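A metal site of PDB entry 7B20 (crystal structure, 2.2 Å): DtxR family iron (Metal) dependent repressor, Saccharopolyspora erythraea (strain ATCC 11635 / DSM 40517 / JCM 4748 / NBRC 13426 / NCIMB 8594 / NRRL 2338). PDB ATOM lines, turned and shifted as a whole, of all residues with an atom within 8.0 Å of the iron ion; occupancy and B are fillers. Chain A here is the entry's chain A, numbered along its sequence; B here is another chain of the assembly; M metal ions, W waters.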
ATOM      1  N   ARG A  15       8.279   2.887  15.938  1.00  0.00           N
ATOM      2  CA  ARG A  15       8.377   3.060  14.467  1.00  0.00           C
ATOM      3  C   ARG A  15       6.973   3.336  13.903  1.00  0.00           C
ATOM      4  O   ARG A  15       6.893   4.151  12.966  1.00  0.00           O
ATOM      5  CB  ARG A  15       9.017   1.844  13.789  1.00  0.00           C
ATOM      6  CG  ARG A  15       9.775   2.208  12.520  1.00  0.00           C
ATOM      7  CD  ARG A  15       9.797   1.089  11.492  1.00  0.00           C
ATOM      8  NE  ARG A  15       8.522   0.962  10.795  1.00  0.00           N
ATOM      9  CZ  ARG A  15       8.063  -0.153  10.229  1.00  0.00           C
ATOM     10  NH1 ARG A  15       8.775  -1.275  10.244  1.00  0.00           N
ATOM     11  NH2 ARG A  15       6.877  -0.143   9.632  1.00  0.00           N
ATOM     12  N   ASP A  19       5.978   6.336  11.615  1.00  0.00           N
ATOM     13  CA  ASP A  19       5.246   6.115  10.341  1.00  0.00           C
ATOM     14  C   ASP A  19       4.098   7.127  10.231  1.00  0.00           C
ATOM     15  O   ASP A  19       4.012   7.809   9.192  1.00  0.00           O
ATOM     16  CB  ASP A  19       4.701   4.687  10.231  1.00  0.00           C
ATOM     17  CG  ASP A  19       5.754   3.596  10.133  1.00  0.00           C
ATOM     18  OD1 ASP A  19       6.930   3.933   9.904  1.00  0.00           O
ATOM     19  OD2 ASP A  19       5.389   2.412  10.297  1.00  0.00           O
ATOM     20  N   MET A  78      14.200   3.071  12.386  1.00  0.00           N
ATOM     21  CA  MET A  78      13.811   3.465  11.008  1.00  0.00           C
ATOM     22  C   MET A  78      15.056   3.469  10.104  1.00  0.00           C
ATOM     23  O   MET A  78      14.952   3.046   8.935  1.00  0.00           O
ATOM     24  CB  MET A  78      13.160   4.849  10.976  1.00  0.00           C
ATOM     25  CG  MET A  78      12.624   5.228   9.610  1.00  0.00           C
ATOM     26  SD  MET A  78      11.411   4.018   9.009  1.00  0.00           S
ATOM     27  CE  MET A  78       9.978   4.525   9.938  1.00  0.00           C
ATOM     28  N   HIS A  81      15.995  -0.049   9.305  1.00  0.00           N
ATOM     29  CA  HIS A  81      14.932  -0.567   8.410  1.00  0.00           C
ATOM     30  C   HIS A  81      15.238  -0.198   6.957  1.00  0.00           C
ATOM     31  O   HIS A  81      15.167  -1.096   6.096  1.00  0.00           O
ATOM     32  CB  HIS A  81      13.561  -0.028   8.849  1.00  0.00           C
ATOM     33  CG  HIS A  81      12.447  -0.444   7.940  1.00  0.00           C
ATOM     34  ND1 HIS A  81      11.853  -1.689   8.028  1.00  0.00           N
ATOM     35  CD2 HIS A  81      11.833   0.203   6.931  1.00  0.00           C
ATOM     36  CE1 HIS A  81      10.921  -1.790   7.094  1.00  0.00           C
ATOM     37  NE2 HIS A  81      10.888  -0.632   6.421  1.00  0.00           N
ATOM     38  N   ARG A  82      15.559   1.077   6.695  1.00  0.00           N
ATOM     39  CA  ARG A  82      15.695   1.616   5.311  1.00  0.00           C
ATOM     40  C   ARG A  82      17.058   1.231   4.726  1.00  0.00           C
ATOM     41  O   ARG A  82      17.129   1.060   3.498  1.00  0.00           O
ATOM     42  CB  ARG A  82      15.429   3.124   5.326  1.00  0.00           C
ATOM     43  CG  ARG A  82      13.954   3.435   5.531  1.00  0.00           C
ATOM     44  CD  ARG A  82      13.577   4.893   5.634  1.00  0.00           C
ATOM     45  NE  ARG A  82      12.112   4.958   5.729  1.00  0.00           N
ATOM     46  CZ  ARG A  82      11.415   5.990   6.166  1.00  0.00           C
ATOM     47  NH1 ARG A  82      12.010   7.111   6.556  1.00  0.00           N
ATOM     48  NH2 ARG A  82      10.097   5.900   6.209  1.00  0.00           N
ATOM     49  N   GLU A  85      16.520  -2.356   3.702  1.00  0.00           N
ATOM     50  CA  GLU A  85      15.748  -2.316   2.430  1.00  0.00           C
ATOM     51  C   GLU A  85      16.698  -2.087   1.250  1.00  0.00           C
ATOM     52  O   GLU A  85      16.575  -2.807   0.245  1.00  0.00           O
ATOM     53  CB  GLU A  85      14.663  -1.242   2.485  1.00  0.00           C
ATOM     54  CG  GLU A  85      13.486  -1.617   3.365  1.00  0.00           C
ATOM     55  CD  GLU A  85      12.351  -0.609   3.367  1.00  0.00           C
ATOM     56  OE1 GLU A  85      12.622   0.599   3.197  1.00  0.00           O
ATOM     57  OE2 GLU A  85      11.189  -1.037   3.526  1.00  0.00           O
ATOM     58  N   VAL A  99      10.299  -6.980   0.297  1.00  0.00           N
ATOM     59  CA  VAL A  99      11.484  -6.377   0.974  1.00  0.00           C
ATOM     60  C   VAL A  99      11.075  -5.779   2.331  1.00  0.00           C
ATOM     61  O   VAL A  99      11.798  -6.030   3.310  1.00  0.00           O
ATOM     62  CB  VAL A  99      12.170  -5.323   0.080  1.00  0.00           C
ATOM     63  CG1 VAL A  99      13.042  -4.366   0.872  1.00  0.00           C
ATOM     64  CG2 VAL A  99      12.972  -5.998  -1.030  1.00  0.00           C
ATOM     65  N   HIS A 100       9.982  -5.010   2.380  1.00  0.00           N
ATOM     66  CA  HIS A 100       9.544  -4.279   3.599  1.00  0.00           C
ATOM     67  C   HIS A 100       9.352  -5.260   4.762  1.00  0.00           C
ATOM     68  O   HIS A 100       9.879  -4.966   5.850  1.00  0.00           O
ATOM     69  CB  HIS A 100       8.265  -3.474   3.335  1.00  0.00           C
ATOM     70  CG  HIS A 100       7.676  -2.921   4.590  1.00  0.00           C
ATOM     71  ND1 HIS A 100       8.208  -1.814   5.230  1.00  0.00           N
ATOM     72  CD2 HIS A 100       6.618  -3.318   5.333  1.00  0.00           C
ATOM     73  CE1 HIS A 100       7.503  -1.561   6.312  1.00  0.00           C
ATOM     74  NE2 HIS A 100       6.527  -2.464   6.401  1.00  0.00           N
ATOM     75  N   LEU A 101       8.642  -6.367   4.540  1.00  0.00           N
ATOM     76  CA  LEU A 101       8.303  -7.354   5.599  1.00  0.00           C
ATOM     77  C   LEU A 101       9.591  -8.012   6.133  1.00  0.00           C
ATOM     78  O   LEU A 101       9.626  -8.334   7.337  1.00  0.00           O
ATOM     79  CB  LEU A 101       7.340  -8.408   5.039  1.00  0.00           C
ATOM     80  CG  LEU A 101       6.883  -9.475   6.035  1.00  0.00           C
ATOM     81  CD1 LEU A 101       6.168  -8.850   7.227  1.00  0.00           C
ATOM     82  CD2 LEU A 101       5.997 -10.512   5.367  1.00  0.00           C
ATOM     83  N   GLU A 102      10.594  -8.185   5.271  1.00  0.00           N
ATOM     84  CA  GLU A 102      11.932  -8.708   5.654  1.00  0.00           C
ATOM     85  C   GLU A 102      12.635  -7.640   6.508  1.00  0.00           C
ATOM     86  O   GLU A 102      13.065  -7.974   7.630  1.00  0.00           O
ATOM     87  CB  GLU A 102      12.766  -9.038   4.415  1.00  0.00           C
ATOM     88  CG  GLU A 102      13.942  -9.956   4.708  1.00  0.00           C
ATOM     89  CD  GLU A 102      13.586 -11.412   4.952  1.00  0.00           C
ATOM     90  OE1 GLU A 102      12.524 -11.854   4.457  1.00  0.00           O
ATOM     91  OE2 GLU A 102      14.367 -12.115   5.625  1.00  0.00           O
ATOM     92  N   ALA A 103      12.724  -6.417   5.993  1.00  0.00           N
ATOM     93  CA  ALA A 103      13.392  -5.254   6.631  1.00  0.00           C
ATOM     94  C   ALA A 103      12.712  -4.915   7.950  1.00  0.00           C
ATOM     95  O   ALA A 103      13.383  -4.360   8.841  1.00  0.00           O
ATOM     96  CB  ALA A 103      13.373  -4.074   5.681  1.00  0.00           C
ATOM     97  N   CYS A 104      11.416  -5.221   8.097  1.00  0.00           N
ATOM     98  CA  CYS A 104      10.613  -4.955   9.322  1.00  0.00           C
ATOM     99  C   CYS A 104      11.104  -5.840  10.468  1.00  0.00           C
ATOM    100  O   CYS A 104      10.957  -5.441  11.628  1.00  0.00           O
ATOM    101  CB  CYS A 104       9.127  -5.174   9.069  1.00  0.00           C
ATOM    102  SG  CYS A 104       8.086  -4.545  10.408  1.00  0.00           S
ATOM    103  N   GLU A 107      15.289  -4.831  11.217  1.00  0.00           N
ATOM    104  CA  GLU A 107      15.487  -3.516  11.885  1.00  0.00           C
ATOM    105  C   GLU A 107      15.770  -3.692  13.382  1.00  0.00           C
ATOM    106  O   GLU A 107      16.369  -2.779  13.974  1.00  0.00           O
ATOM    107  CB  GLU A 107      14.265  -2.605  11.658  1.00  0.00           C
ATOM    108  CG  GLU A 107      13.012  -3.053  12.398  1.00  0.00           C
ATOM    109  CD  GLU A 107      11.720  -2.412  11.930  1.00  0.00           C
ATOM    110  OE1 GLU A 107      11.759  -1.657  10.944  1.00  0.00           O
ATOM    111  OE2 GLU A 107      10.671  -2.671  12.545  1.00  0.00           O
ATOM    112  N   SER A 128      15.501   5.274   1.072  1.00  0.00           N
ATOM    113  CA  SER A 128      15.164   3.829   0.893  1.00  0.00           C
ATOM    114  C   SER A 128      14.861   3.585  -0.588  1.00  0.00           C
ATOM    115  O   SER A 128      14.750   4.544  -1.359  1.00  0.00           O
ATOM    116  CB  SER A 128      14.010   3.431   1.778  1.00  0.00           C
ATOM    117  OG  SER A 128      12.760   3.813   1.213  1.00  0.00           O
ATOM    118  N   PRO A 129      14.704   2.324  -1.021  1.00  0.00           N
ATOM    119  CA  PRO A 129      14.271   2.032  -2.398  1.00  0.00           C
ATOM    120  C   PRO A 129      12.905   2.642  -2.759  1.00  0.00           C
ATOM    121  O   PRO A 129      12.644   2.799  -3.937  1.00  0.00           O
ATOM    122  CB  PRO A 129      14.195   0.494  -2.448  1.00  0.00           C
ATOM    123  CG  PRO A 129      15.093   0.029  -1.315  1.00  0.00           C
ATOM    124  CD  PRO A 129      14.949   1.103  -0.249  1.00  0.00           C
ATOM    125  N   TYR A 130      12.084   2.972  -1.753  1.00  0.00           N
ATOM    126  CA  TYR A 130      10.694   3.490  -1.912  1.00  0.00           C
ATOM    127  C   TYR A 130      10.687   5.016  -1.743  1.00  0.00           C
ATOM    128  O   TYR A 130       9.600   5.586  -1.597  1.00  0.00           O
ATOM    129  CB  TYR A 130       9.771   2.784  -0.913  1.00  0.00           C
ATOM    130  CG  TYR A 130       9.941   1.292  -0.923  1.00  0.00           C
ATOM    131  CD1 TYR A 130       9.442   0.525  -1.963  1.00  0.00           C
ATOM    132  CD2 TYR A 130      10.636   0.640   0.094  1.00  0.00           C
ATOM    133  CE1 TYR A 130       9.616  -0.848  -1.993  1.00  0.00           C
ATOM    134  CE2 TYR A 130      10.812  -0.732   0.074  1.00  0.00           C
ATOM    135  CZ  TYR A 130      10.298  -1.481  -0.973  1.00  0.00           C
ATOM    136  OH  TYR A 130      10.474  -2.832  -0.995  1.00  0.00           O
ATOM    137  N   ASN A 132      11.780   7.056   0.574  1.00  0.00           N
ATOM    138  CA  ASN A 132      11.660   7.594   1.956  1.00  0.00           C
ATOM    139  C   ASN A 132      13.049   7.964   2.465  1.00  0.00           C
ATOM    140  O   ASN A 132      13.956   7.131   2.423  1.00  0.00           O
ATOM    141  CB  ASN A 132      10.963   6.602   2.900  1.00  0.00           C
ATOM    142  CG  ASN A 132       9.567   6.258   2.443  1.00  0.00           C
ATOM    143  OD1 ASN A 132       8.718   7.133   2.288  1.00  0.00           O
ATOM    144  ND2 ASN A 132       9.309   4.971   2.228  1.00  0.00           N
ATOM    145  N   ILE B 172       6.928   6.441  -1.254  1.00  0.00           N
ATOM    146  CA  ILE B 172       5.861   5.448  -0.902  1.00  0.00           C
ATOM    147  C   ILE B 172       6.082   5.032   0.558  1.00  0.00           C
ATOM    148  O   ILE B 172       7.050   4.303   0.813  1.00  0.00           O
ATOM    149  CB  ILE B 172       5.891   4.235  -1.873  1.00  0.00           C
ATOM    150  CG1 ILE B 172       5.732   4.678  -3.332  1.00  0.00           C
ATOM    151  CG2 ILE B 172       4.842   3.210  -1.472  1.00  0.00           C
ATOM    152  CD1 ILE B 172       5.878   3.560  -4.334  1.00  0.00           C
ATOM    153  N   ALA B 173       5.218   5.498   1.462  1.00  0.00           N
ATOM    154  CA  ALA B 173       5.348   5.357   2.927  1.00  0.00           C
ATOM    155  C   ALA B 173       5.241   3.878   3.330  1.00  0.00           C
ATOM    156  O   ALA B 173       4.778   3.061   2.503  1.00  0.00           O
ATOM    157  CB  ALA B 173       4.311   6.186   3.634  1.00  0.00           C
ATOM    158  N   GLU B 174       5.633   3.568   4.576  1.00  0.00           N
ATOM    159  CA  GLU B 174       5.711   2.189   5.128  1.00  0.00           C
ATOM    160  C   GLU B 174       4.301   1.583   5.205  1.00  0.00           C
ATOM    161  O   GLU B 174       4.185   0.344   5.124  1.00  0.00           O
ATOM    162  CB  GLU B 174       6.373   2.195   6.512  1.00  0.00           C
ATOM    163  CG  GLU B 174       7.738   2.875   6.556  1.00  0.00           C
ATOM    164  CD  GLU B 174       8.820   2.260   5.684  1.00  0.00           C
ATOM    165  OE1 GLU B 174       9.810   2.955   5.408  1.00  0.00           O
ATOM    166  OE2 GLU B 174       8.677   1.083   5.303  1.00  0.00           O
ATOM    167  N   HIS B 175       3.266   2.427   5.368  1.00  0.00           N
ATOM    168  CA  HIS B 175       1.832   2.036   5.384  1.00  0.00           C
ATOM    169  C   HIS B 175       1.463   1.327   4.073  1.00  0.00           C
ATOM    170  O   HIS B 175       0.748   0.311   4.147  1.00  0.00           O
ATOM    171  CB  HIS B 175       0.959   3.276   5.637  1.00  0.00           C
ATOM    172  CG  HIS B 175      -0.515   3.022   5.561  1.00  0.00           C
ATOM    173  ND1 HIS B 175      -1.123   1.979   6.222  1.00  0.00           N
ATOM    174  CD2 HIS B 175      -1.499   3.684   4.918  1.00  0.00           C
ATOM    175  CE1 HIS B 175      -2.425   2.001   5.981  1.00  0.00           C
ATOM    176  NE2 HIS B 175      -2.684   3.041   5.184  1.00  0.00           N
ATOM    177  N   VAL B 176       1.930   1.844   2.939  1.00  0.00           N
ATOM    178  CA  VAL B 176       1.622   1.310   1.575  1.00  0.00           C
ATOM    179  C   VAL B 176       2.368  -0.014   1.376  1.00  0.00           C
ATOM    180  O   VAL B 176       1.795  -0.934   0.766  1.00  0.00           O
ATOM    181  CB  VAL B 176       1.971   2.316   0.470  1.00  0.00           C
ATOM    182  CG1 VAL B 176       1.642   1.775  -0.918  1.00  0.00           C
ATOM    183  CG2 VAL B 176       1.301   3.662   0.687  1.00  0.00           C
ATOM    184  N   GLN B 177       3.597  -0.098   1.893  1.00  0.00           N
ATOM    185  CA  GLN B 177       4.519  -1.257   1.704  1.00  0.00           C
ATOM    186  C   GLN B 177       3.958  -2.507   2.409  1.00  0.00           C
ATOM    187  O   GLN B 177       4.320  -3.619   1.981  1.00  0.00           O
ATOM    188  CB  GLN B 177       5.909  -0.916   2.236  1.00  0.00           C
ATOM    189  CG  GLN B 177       6.594   0.218   1.493  1.00  0.00           C
ATOM    190  CD  GLN B 177       7.868   0.662   2.177  1.00  0.00           C
ATOM    191  OE1 GLN B 177       8.641  -0.144   2.672  1.00  0.00           O
ATOM    192  NE2 GLN B 177       8.110   1.969   2.186  1.00  0.00           N
ATOM    193  N   LEU B 178       3.113  -2.333   3.434  1.00  0.00           N
ATOM    194  CA  LEU B 178       2.576  -3.437   4.288  1.00  0.00           C
ATOM    195  C   LEU B 178       1.652  -4.358   3.487  1.00  0.00           C
ATOM    196  O   LEU B 178       1.399  -5.483   3.969  1.00  0.00           O
ATOM    197  CB  LEU B 178       1.846  -2.846   5.498  1.00  0.00           C
ATOM    198  CG  LEU B 178       2.692  -2.664   6.753  1.00  0.00           C
ATOM    199  CD1 LEU B 178       2.027  -1.710   7.740  1.00  0.00           C
ATOM    200  CD2 LEU B 178       2.983  -4.002   7.407  1.00  0.00           C
ATOM    201  N   MET B 183       1.567  -3.431  -3.708  1.00  0.00           N
ATOM    202  CA  MET B 183       2.923  -3.000  -4.132  1.00  0.00           C
ATOM    203  C   MET B 183       3.251  -3.608  -5.507  1.00  0.00           C
ATOM    204  O   MET B 183       3.817  -2.879  -6.341  1.00  0.00           O
ATOM    205  CB  MET B 183       3.989  -3.391  -3.106  1.00  0.00           C
ATOM    206  CG  MET B 183       3.979  -2.537  -1.853  1.00  0.00           C
ATOM    207  SD  MET B 183       4.473  -0.810  -2.157  1.00  0.00           S
ATOM    208  CE  MET B 183       6.241  -0.988  -2.332  1.00  0.00           C
HETATM  209 FE    FE M   1       9.619  -0.358   4.555  1.00  0.00          FE
HETATM  210  O   HOH W   1      10.826   2.538   3.111  1.00  0.00           O
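OE1 of Glu 174 of chain B is in salt-bridge range of NH2 of Arg 82 (3.1 Å).
ND1 of His 81 sits at hydrogen-bond distance from OE1 of Glu 107, at 2.9 Å.
A ring nitrogen (ND1) of His 81 lies within hydrogen-bond range of the backbone carbonyl oxygen of Ala 103.
The side-chain amide nitrogen of Gln 177 of chain B sits at hydrogen-bond distance from the backbone carbonyl oxygen of Ile 172 of chain B (2.9 Å).
The side-chain amide nitrogen (ND2) of Asn 132 lies close to the side-chain amide nitrogen (NE2) of Gln 177 of chain B (3.2 Å).
Five residues have an atom within 4 Å of the iron ion: His 81, Glu 85, His 100, Glu 174 of chain B and Gln 177 of chain B.
The iron ion is bound by OE2 of Glu 174 of chain B (1.9 Å), OE2 of Glu 85 (2.0 Å), OE1 of Gln 177 of chain B (2.1 Å), ND1 of His 100 (2.1 Å) and NE2 of His 81 (2.3 Å).
The iron ion has five donor atoms within binding distance.
Water W1 lies within hydrogen-bond range of OE1 of Glu 174 of chain B (2.5 Å), OE1 of Glu 85 (2.6 Å), NE2 of Gln 177 of chain B (2.9 Å), OG of Ser 128 (3.0 Å) and ND2 of Asn 132 (3.0 Å).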
